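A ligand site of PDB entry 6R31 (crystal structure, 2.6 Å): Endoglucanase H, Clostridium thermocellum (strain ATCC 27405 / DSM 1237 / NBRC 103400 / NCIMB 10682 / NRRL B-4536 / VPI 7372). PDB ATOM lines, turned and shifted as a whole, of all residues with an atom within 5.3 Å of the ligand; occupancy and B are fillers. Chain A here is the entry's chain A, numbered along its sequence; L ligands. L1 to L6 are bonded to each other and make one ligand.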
ATOM      1  N   TYR A  22      12.346  22.685   0.795  1.00  0.00           N
ATOM      2  CA  TYR A  22      11.510  23.579   0.003  1.00  0.00           C
ATOM      3  C   TYR A  22      11.390  24.909   0.744  1.00  0.00           C
ATOM      4  O   TYR A  22      11.547  24.947   1.960  1.00  0.00           O
ATOM      5  CB  TYR A  22      10.144  22.930  -0.315  1.00  0.00           C
ATOM      6  CG  TYR A  22       9.338  22.494   0.884  1.00  0.00           C
ATOM      7  CD1 TYR A  22       8.566  23.406   1.601  1.00  0.00           C
ATOM      8  CD2 TYR A  22       9.364  21.183   1.326  1.00  0.00           C
ATOM      9  CE1 TYR A  22       7.837  23.021   2.709  1.00  0.00           C
ATOM     10  CE2 TYR A  22       8.626  20.779   2.434  1.00  0.00           C
ATOM     11  CZ  TYR A  22       7.849  21.705   3.131  1.00  0.00           C
ATOM     12  OH  TYR A  22       7.118  21.342   4.218  1.00  0.00           O
ATOM     13  N   GLU A  25       9.188  32.811  -1.044  1.00  0.00           N
ATOM     14  CA  GLU A  25       8.933  34.196  -0.671  1.00  0.00           C
ATOM     15  C   GLU A  25       9.930  34.662   0.376  1.00  0.00           C
ATOM     16  O   GLU A  25       9.542  35.100   1.460  1.00  0.00           O
ATOM     17  CB  GLU A  25       7.513  34.367  -0.175  1.00  0.00           C
ATOM     18  CG  GLU A  25       6.482  33.895  -1.171  1.00  0.00           C
ATOM     19  CD  GLU A  25       5.101  34.028  -0.575  1.00  0.00           C
ATOM     20  OE1 GLU A  25       4.534  35.152  -0.654  1.00  0.00           O
ATOM     21  OE2 GLU A  25       4.622  33.026   0.023  1.00  0.00           O
ATOM     22  N   ASP A  51       6.060  36.640   5.314  1.00  0.00           N
ATOM     23  CA  ASP A  51       5.087  36.077   4.388  1.00  0.00           C
ATOM     24  C   ASP A  51       5.500  34.683   3.902  1.00  0.00           C
ATOM     25  O   ASP A  51       4.665  33.977   3.354  1.00  0.00           O
ATOM     26  CB  ASP A  51       4.845  37.034   3.214  1.00  0.00           C
ATOM     27  CG  ASP A  51       4.228  38.344   3.674  1.00  0.00           C
ATOM     28  OD1 ASP A  51       3.312  38.282   4.553  1.00  0.00           O
ATOM     29  OD2 ASP A  51       4.663  39.413   3.176  1.00  0.00           O
ATOM     30  N   GLY A  52       6.777  34.294   4.111  1.00  0.00           N
ATOM     31  CA  GLY A  52       7.327  33.109   3.471  1.00  0.00           C
ATOM     32  C   GLY A  52       7.171  31.844   4.315  1.00  0.00           C
ATOM     33  O   GLY A  52       6.488  31.854   5.338  1.00  0.00           O
ATOM     34  N   TYR A  53       7.851  30.769   3.891  1.00  0.00           N
ATOM     35  CA  TYR A  53       7.724  29.454   4.495  1.00  0.00           C
ATOM     36  C   TYR A  53       8.978  28.647   4.158  1.00  0.00           C
ATOM     37  O   TYR A  53       9.659  28.947   3.182  1.00  0.00           O
ATOM     38  CB  TYR A  53       6.483  28.723   3.955  1.00  0.00           C
ATOM     39  CG  TYR A  53       6.443  28.517   2.458  1.00  0.00           C
ATOM     40  CD1 TYR A  53       5.916  29.489   1.619  1.00  0.00           C
ATOM     41  CD2 TYR A  53       6.953  27.363   1.878  1.00  0.00           C
ATOM     42  CE1 TYR A  53       5.904  29.316   0.251  1.00  0.00           C
ATOM     43  CE2 TYR A  53       6.933  27.172   0.510  1.00  0.00           C
ATOM     44  CZ  TYR A  53       6.411  28.153  -0.309  1.00  0.00           C
ATOM     45  OH  TYR A  53       6.396  27.950  -1.657  1.00  0.00           O
ATOM     46  N   VAL A  57      11.664  17.594   4.133  1.00  0.00           N
ATOM     47  CA  VAL A  57      10.640  16.583   3.882  1.00  0.00           C
ATOM     48  C   VAL A  57      11.261  15.229   3.542  1.00  0.00           C
ATOM     49  O   VAL A  57      12.179  15.149   2.745  1.00  0.00           O
ATOM     50  CB  VAL A  57       9.644  17.038   2.797  1.00  0.00           C
ATOM     51  CG1 VAL A  57      10.320  17.433   1.490  1.00  0.00           C
ATOM     52  CG2 VAL A  57       8.545  16.007   2.547  1.00  0.00           C
ATOM     53  N   SER A  59       9.565  11.646   2.106  1.00  0.00           N
ATOM     54  CA  SER A  59       8.419  10.906   1.604  1.00  0.00           C
ATOM     55  C   SER A  59       8.671   9.422   1.822  1.00  0.00           C
ATOM     56  O   SER A  59       9.616   8.862   1.269  1.00  0.00           O
ATOM     57  CB  SER A  59       8.173  11.212   0.146  1.00  0.00           C
ATOM     58  OG  SER A  59       7.877  12.595  -0.041  1.00  0.00           O
ATOM     59  N   MET A  88       5.558  17.747  11.251  1.00  0.00           N
ATOM     60  CA  MET A  88       4.315  17.476  10.548  1.00  0.00           C
ATOM     61  C   MET A  88       4.259  16.095   9.891  1.00  0.00           C
ATOM     62  O   MET A  88       5.188  15.672   9.206  1.00  0.00           O
ATOM     63  CB  MET A  88       4.027  18.522   9.464  1.00  0.00           C
ATOM     64  CG  MET A  88       3.077  17.990   8.417  1.00  0.00           C
ATOM     65  SD  MET A  88       2.520  19.290   7.346  1.00  0.00           S
ATOM     66  CE  MET A  88       3.842  19.316   6.130  1.00  0.00           C
ATOM     67  N   GLY A  98       0.412  15.640  -5.444  1.00  0.00           N
ATOM     68  CA  GLY A  98       0.681  16.385  -4.226  1.00  0.00           C
ATOM     69  C   GLY A  98       0.523  15.512  -2.975  1.00  0.00           C
ATOM     70  O   GLY A  98       0.571  14.292  -3.075  1.00  0.00           O
ATOM     71  N   ASP A  99       0.331  16.137  -1.796  1.00  0.00           N
ATOM     72  CA  ASP A  99       0.123  15.396  -0.566  1.00  0.00           C
ATOM     73  C   ASP A  99      -1.295  15.621  -0.050  1.00  0.00           C
ATOM     74  O   ASP A  99      -2.139  16.179  -0.749  1.00  0.00           O
ATOM     75  CB  ASP A  99       1.243  15.652   0.451  1.00  0.00           C
ATOM     76  CG  ASP A  99       1.461  17.108   0.824  1.00  0.00           C
ATOM     77  OD1 ASP A  99       0.556  17.932   0.514  1.00  0.00           O
ATOM     78  OD2 ASP A  99       2.535  17.422   1.430  1.00  0.00           O
ATOM     79  N   HIS A 102      -2.734  17.742   6.560  1.00  0.00           N
ATOM     80  CA  HIS A 102      -1.526  18.053   7.335  1.00  0.00           C
ATOM     81  C   HIS A 102      -1.823  18.049   8.831  1.00  0.00           C
ATOM     82  O   HIS A 102      -2.774  18.698   9.273  1.00  0.00           O
ATOM     83  CB  HIS A 102      -0.989  19.439   6.972  1.00  0.00           C
ATOM     84  CG  HIS A 102      -0.302  19.521   5.648  1.00  0.00           C
ATOM     85  ND1 HIS A 102      -0.153  20.716   4.974  1.00  0.00           N
ATOM     86  CD2 HIS A 102       0.278  18.574   4.885  1.00  0.00           C
ATOM     87  CE1 HIS A 102       0.491  20.503   3.843  1.00  0.00           C
ATOM     88  NE2 HIS A 102       0.779  19.206   3.769  1.00  0.00           N
ATOM     89  N   ARG A 126      -3.609  20.985  10.930  1.00  0.00           N
ATOM     90  CA  ARG A 126      -2.996  22.249  10.587  1.00  0.00           C
ATOM     91  C   ARG A 126      -4.044  23.313  10.268  1.00  0.00           C
ATOM     92  O   ARG A 126      -4.947  23.094   9.467  1.00  0.00           O
ATOM     93  CB  ARG A 126      -2.019  22.092   9.419  1.00  0.00           C
ATOM     94  CG  ARG A 126      -1.189  23.347   9.162  1.00  0.00           C
ATOM     95  CD  ARG A 126      -0.135  23.212   8.073  1.00  0.00           C
ATOM     96  NE  ARG A 126       0.539  24.484   7.868  1.00  0.00           N
ATOM     97  CZ  ARG A 126       1.327  24.778   6.830  1.00  0.00           C
ATOM     98  NH1 ARG A 126       1.547  23.892   5.874  1.00  0.00           N
ATOM     99  NH2 ARG A 126       1.863  25.983   6.759  1.00  0.00           N
ATOM    100  N   ASP A 128      -3.271  26.826   9.512  1.00  0.00           N
ATOM    101  CA  ASP A 128      -2.858  27.909   8.624  1.00  0.00           C
ATOM    102  C   ASP A 128      -2.944  27.504   7.149  1.00  0.00           C
ATOM    103  O   ASP A 128      -3.092  28.391   6.304  1.00  0.00           O
ATOM    104  CB  ASP A 128      -1.512  28.512   8.993  1.00  0.00           C
ATOM    105  CG  ASP A 128      -0.361  27.516   8.989  1.00  0.00           C
ATOM    106  OD1 ASP A 128      -0.608  26.337   9.275  1.00  0.00           O
ATOM    107  OD2 ASP A 128       0.782  27.937   8.714  1.00  0.00           O
ATOM    108  N   TYR A 129      -2.852  26.194   6.839  1.00  0.00           N
ATOM    109  CA  TYR A 129      -2.786  25.733   5.451  1.00  0.00           C
ATOM    110  C   TYR A 129      -3.241  24.279   5.323  1.00  0.00           C
ATOM    111  O   TYR A 129      -2.912  23.429   6.144  1.00  0.00           O
ATOM    112  CB  TYR A 129      -1.378  25.951   4.862  1.00  0.00           C
ATOM    113  CG  TYR A 129      -1.154  25.428   3.462  1.00  0.00           C
ATOM    114  CD1 TYR A 129      -1.423  26.202   2.340  1.00  0.00           C
ATOM    115  CD2 TYR A 129      -0.694  24.128   3.244  1.00  0.00           C
ATOM    116  CE1 TYR A 129      -1.234  25.719   1.050  1.00  0.00           C
ATOM    117  CE2 TYR A 129      -0.499  23.633   1.975  1.00  0.00           C
ATOM    118  CZ  TYR A 129      -0.773  24.419   0.863  1.00  0.00           C
ATOM    119  OH  TYR A 129      -0.568  23.897  -0.387  1.00  0.00           O
ATOM    120  N   PRO A 131      -3.357  21.413   1.789  1.00  0.00           N
ATOM    121  CA  PRO A 131      -3.042  21.332   0.363  1.00  0.00           C
ATOM    122  C   PRO A 131      -4.314  20.953  -0.389  1.00  0.00           C
ATOM    123  O   PRO A 131      -5.287  20.483   0.204  1.00  0.00           O
ATOM    124  CB  PRO A 131      -2.003  20.212   0.333  1.00  0.00           C
ATOM    125  CG  PRO A 131      -2.448  19.269   1.430  1.00  0.00           C
ATOM    126  CD  PRO A 131      -3.059  20.159   2.505  1.00  0.00           C
ATOM    127  N   ASP A 146       1.809   9.820   3.922  1.00  0.00           N
ATOM    128  CA  ASP A 146       2.698  10.122   2.812  1.00  0.00           C
ATOM    129  C   ASP A 146       4.094  10.518   3.311  1.00  0.00           C
ATOM    130  O   ASP A 146       5.086   9.960   2.867  1.00  0.00           O
ATOM    131  CB  ASP A 146       2.103  11.189   1.894  1.00  0.00           C
ATOM    132  CG  ASP A 146       3.093  11.709   0.870  1.00  0.00           C
ATOM    133  OD1 ASP A 146       3.471  10.928  -0.041  1.00  0.00           O
ATOM    134  OD2 ASP A 146       3.505  12.876   1.002  1.00  0.00           O
ATOM    135  N   SER A 147       4.156  11.494   4.232  1.00  0.00           N
ATOM    136  CA  SER A 147       5.415  12.200   4.451  1.00  0.00           C
ATOM    137  C   SER A 147       5.495  12.836   5.835  1.00  0.00           C
ATOM    138  O   SER A 147       4.493  13.323   6.370  1.00  0.00           O
ATOM    139  CB  SER A 147       5.610  13.246   3.388  1.00  0.00           C
ATOM    140  OG  SER A 147       4.484  14.108   3.282  1.00  0.00           O
ATOM    141  N   HIS A 149       7.744  15.896   8.075  1.00  0.00           N
ATOM    142  CA  HIS A 149       8.473  17.143   7.860  1.00  0.00           C
ATOM    143  C   HIS A 149       8.922  17.797   9.166  1.00  0.00           C
ATOM    144  O   HIS A 149       8.257  17.678  10.200  1.00  0.00           O
ATOM    145  CB  HIS A 149       7.619  18.212   7.187  1.00  0.00           C
ATOM    146  CG  HIS A 149       6.812  17.756   6.026  1.00  0.00           C
ATOM    147  ND1 HIS A 149       6.922  18.354   4.788  1.00  0.00           N
ATOM    148  CD2 HIS A 149       5.841  16.833   5.913  1.00  0.00           C
ATOM    149  CE1 HIS A 149       6.072  17.792   3.960  1.00  0.00           C
ATOM    150  NE2 HIS A 149       5.399  16.846   4.621  1.00  0.00           N
ATOM    151  N   MET A 151       9.427  21.907   9.800  1.00  0.00           N
ATOM    152  CA  MET A 151       9.002  23.098   9.067  1.00  0.00           C
ATOM    153  C   MET A 151       8.792  24.297  10.001  1.00  0.00           C
ATOM    154  O   MET A 151       8.799  24.151  11.213  1.00  0.00           O
ATOM    155  CB  MET A 151       7.704  22.807   8.305  1.00  0.00           C
ATOM    156  CG  MET A 151       6.517  22.582   9.220  1.00  0.00           C
ATOM    157  SD  MET A 151       4.983  22.209   8.343  1.00  0.00           S
ATOM    158  CE  MET A 151       4.097  23.758   8.556  1.00  0.00           C
ATOM    159  N   TYR A 152       8.549  25.474   9.375  1.00  0.00           N
ATOM    160  CA  TYR A 152       8.427  26.781   9.996  1.00  0.00           C
ATOM    161  C   TYR A 152       7.220  26.873  10.929  1.00  0.00           C
ATOM    162  O   TYR A 152       6.192  26.238  10.714  1.00  0.00           O
ATOM    163  CB  TYR A 152       8.330  27.883   8.918  1.00  0.00           C
ATOM    164  CG  TYR A 152       6.945  28.118   8.353  1.00  0.00           C
ATOM    165  CD1 TYR A 152       6.345  27.189   7.532  1.00  0.00           C
ATOM    166  CD2 TYR A 152       6.229  29.262   8.677  1.00  0.00           C
ATOM    167  CE1 TYR A 152       5.062  27.380   7.035  1.00  0.00           C
ATOM    168  CE2 TYR A 152       4.953  29.470   8.189  1.00  0.00           C
ATOM    169  CZ  TYR A 152       4.372  28.534   7.359  1.00  0.00           C
ATOM    170  OH  TYR A 152       3.106  28.738   6.861  1.00  0.00           O
HETATM  171  C1  LIG L   1       7.800  17.517  -2.013  1.00  0.00           C
HETATM  172  C2  LIG L   1       6.563  17.961  -1.263  1.00  0.00           C
HETATM  173  C3  LIG L   1       5.624  16.853  -1.665  1.00  0.00           C
HETATM  174  C4  LIG L   1       6.025  15.585  -0.971  1.00  0.00           C
HETATM  175  C5  LIG L   1       4.933  14.541  -1.111  1.00  0.00           C
HETATM  176  C6  LIG L   1       8.168  16.116  -1.607  1.00  0.00           C
HETATM  177  O1  LIG L   1       9.155  15.608  -2.452  1.00  0.00           O
HETATM  178  O2  LIG L   1       8.911  18.335  -1.791  1.00  0.00           O
HETATM  179  O3  LIG L   1       6.078  19.160  -1.794  1.00  0.00           O
HETATM  180  O4  LIG L   1       4.235  17.178  -1.601  1.00  0.00           O
HETATM  181  O5  LIG L   1       7.116  15.208  -1.719  1.00  0.00           O
HETATM  182  O6  LIG L   1       5.259  13.348  -1.807  1.00  0.00           O
HETATM  183  C1  LG2 L   2       6.038  21.487  -1.734  1.00  0.00           C
HETATM  184  C2  LG2 L   2       5.863  22.691  -0.851  1.00  0.00           C
HETATM  185  C3  LG2 L   2       4.847  22.448   0.251  1.00  0.00           C
HETATM  186  C4  LG2 L   2       5.195  21.137   0.926  1.00  0.00           C
HETATM  187  C5  LG2 L   2       4.145  20.609   1.881  1.00  0.00           C
HETATM  188  C6  LG2 L   2       6.296  20.240  -0.957  1.00  0.00           C
HETATM  189  O1  LG2 L   2       7.173  21.760  -2.488  1.00  0.00           O
HETATM  190  O2  LG2 L   2       5.534  23.737  -1.734  1.00  0.00           O
HETATM  191  O3  LG2 L   2       4.910  23.447   1.232  1.00  0.00           O
HETATM  192  O4  LG2 L   2       5.330  20.114  -0.017  1.00  0.00           O
HETATM  193  O5  LG2 L   2       2.980  20.367   1.146  1.00  0.00           O
HETATM  194  C1  LG3 L   3       3.771  24.933   2.581  1.00  0.00           C
HETATM  195  C2  LG3 L   3       2.596  25.852   2.615  1.00  0.00           C
HETATM  196  C3  LG3 L   3       2.627  26.828   1.456  1.00  0.00           C
HETATM  197  C4  LG3 L   3       2.828  26.055   0.189  1.00  0.00           C
HETATM  198  C5  LG3 L   3       3.116  26.993  -0.915  1.00  0.00           C
HETATM  199  C6  LG3 L   3       3.737  24.200   1.278  1.00  0.00           C
HETATM  200  O1  LG3 L   3       3.672  24.074   3.671  1.00  0.00           O
HETATM  201  O2  LG3 L   3       2.756  26.525   3.807  1.00  0.00           O
HETATM  202  O3  LG3 L   3       1.415  27.574   1.313  1.00  0.00           O
HETATM  203  O4  LG3 L   3       3.905  25.206   0.335  1.00  0.00           O
HETATM  204  O5  LG3 L   3       3.235  26.303  -2.102  1.00  0.00           O
HETATM  205  C1  LG4 L   4       0.375  29.653   0.814  1.00  0.00           C
HETATM  206  C2  LG4 L   4       0.455  31.133   0.810  1.00  0.00           C
HETATM  207  C3  LG4 L   4       0.886  31.598   2.198  1.00  0.00           C
HETATM  208  C4  LG4 L   4       1.991  30.700   2.795  1.00  0.00           C
HETATM  209  C5  LG4 L   4       2.386  30.963   4.245  1.00  0.00           C
HETATM  210  C6  LG4 L   4       1.593  28.977   1.367  1.00  0.00           C
HETATM  211  O1  LG4 L   4       0.214  29.318  -0.520  1.00  0.00           O
HETATM  212  O2  LG4 L   4      -0.833  31.578   0.371  1.00  0.00           O
HETATM  213  O3  LG4 L   4       1.372  32.936   2.157  1.00  0.00           O
HETATM  214  O4  LG4 L   4       1.650  29.348   2.693  1.00  0.00           O
HETATM  215  O5  LG4 L   4       1.302  31.404   5.042  1.00  0.00           O
HETATM  216  C1  LG5 L   5      -2.172  32.629  -1.343  1.00  0.00           C
HETATM  217  C2  LG5 L   5      -2.217  33.584  -2.511  1.00  0.00           C
HETATM  218  C3  LG5 L   5      -1.538  34.897  -2.185  1.00  0.00           C
HETATM  219  C4  LG5 L   5      -0.268  34.596  -1.437  1.00  0.00           C
HETATM  220  C5  LG5 L   5       0.247  35.878  -0.858  1.00  0.00           C
HETATM  221  C6  LG5 L   5      -0.816  32.451  -0.767  1.00  0.00           C
HETATM  222  O1  LG5 L   5      -2.657  31.434  -1.863  1.00  0.00           O
HETATM  223  O2  LG5 L   5      -3.574  33.777  -2.896  1.00  0.00           O
HETATM  224  O3  LG5 L   5      -1.168  35.532  -3.368  1.00  0.00           O
HETATM  225  O4  LG5 L   5      -0.511  33.737  -0.375  1.00  0.00           O
HETATM  226  O5  LG5 L   5       1.594  35.711  -0.483  1.00  0.00           O
HETATM  227  C1  LG6 L   6      -1.228  37.448  -4.614  1.00  0.00           C
HETATM  228  C2  LG6 L   6      -2.045  38.705  -4.880  1.00  0.00           C
HETATM  229  C3  LG6 L   6      -3.466  38.345  -5.239  1.00  0.00           C
HETATM  230  C4  LG6 L   6      -4.070  37.440  -4.189  1.00  0.00           C
HETATM  231  C5  LG6 L   6      -5.472  36.982  -4.608  1.00  0.00           C
HETATM  232  C6  LG6 L   6      -1.917  36.693  -3.514  1.00  0.00           C
HETATM  233  O1  LG6 L   6       0.129  37.663  -4.182  1.00  0.00           O
HETATM  234  O2  LG6 L   6      -1.539  39.489  -5.937  1.00  0.00           O
HETATM  235  O3  LG6 L   6      -4.244  39.511  -5.244  1.00  0.00           O
HETATM  236  O4  LG6 L   6      -3.206  36.360  -3.916  1.00  0.00           O
HETATM  237  O5  LG6 L   6      -5.561  35.694  -5.195  1.00  0.00           O
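CE1 of Tyr 22 touches O3 of LG2 L2 (3.3 Å).
O of Asp 51 touches O3 of LG4 L4 (3.7 Å).
OH of Tyr 53 touches C5 of LG3 L3, 3.5 Å away.
Val 57 touches the ligand.
NE2 of His 102 touches O5 of LG2 L2, at 3.6 Å.
CE1 of Tyr 129 touches O3 of LG3 L3 (3.2 Å).
CE1 of His 149 touches C5 of LG2 L2 (3.996 Å).
OH of Tyr 152 touches C5 of LG4 L4, 3.5 Å away.
Hydrophobic or aromatic side chains within 4 Å of the ligand: Tyr 22, Tyr 53, Val 57, His 102, Tyr 129 and His 149.
Of the 20 residues printed, 13 come within 4 Å of the ligand.
OD2 of Asp 99 is in hydrogen-bond range of NE2 of His 102.
The side-chain carboxylate (OD2) of Asp 146 sits at hydrogen-bond distance from the side-chain hydroxyl (OG) of Ser 147 (2.8 Å).
OH of Tyr 152 is in hydrogen-bond range of NH2 of Arg 126, 3.0 Å away.
The backbone NH of Arg 126 sits at hydrogen-bond distance from the backbone carbonyl oxygen of His 102 (2.9 Å).
NE of Arg 126 is in salt-bridge range of OD1 of Asp 128 (2.6 Å).
The side-chain carboxylate (OD2) of Asp 128 sits at hydrogen-bond distance from the side-chain hydroxyl (OH) of Tyr 152, 3.1 Å away.
A ring nitrogen (NE2) of His 149 sits at hydrogen-bond distance from the side-chain hydroxyl of Ser 147 (3.2 Å).
The backbone carbonyl oxygen (O) of Met 88 lies within hydrogen-bond range of the backbone NH (N) of His 149 (2.8 Å).
An oxygen (O5) of LG2 L2 lies within hydrogen-bond range of the side-chain carboxylate of Asp 99 (3.0 Å).
OE1 of Glu 25 is in hydrogen-bond range of O5 of LG5 L5.
The side-chain carboxylate (OD2) of Asp 146 sits close to an oxygen (O6) of LIG L1 (3.3 Å).
The guanidinium group (NH1) of Arg 126 sits at hydrogen-bond distance from an oxygen (O1) of LG3 L3 (3.1 Å).
An oxygen (O5) of LIG L1 lies within hydrogen-bond range of the side-chain hydroxyl of Ser 59, 3.2 Å away.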
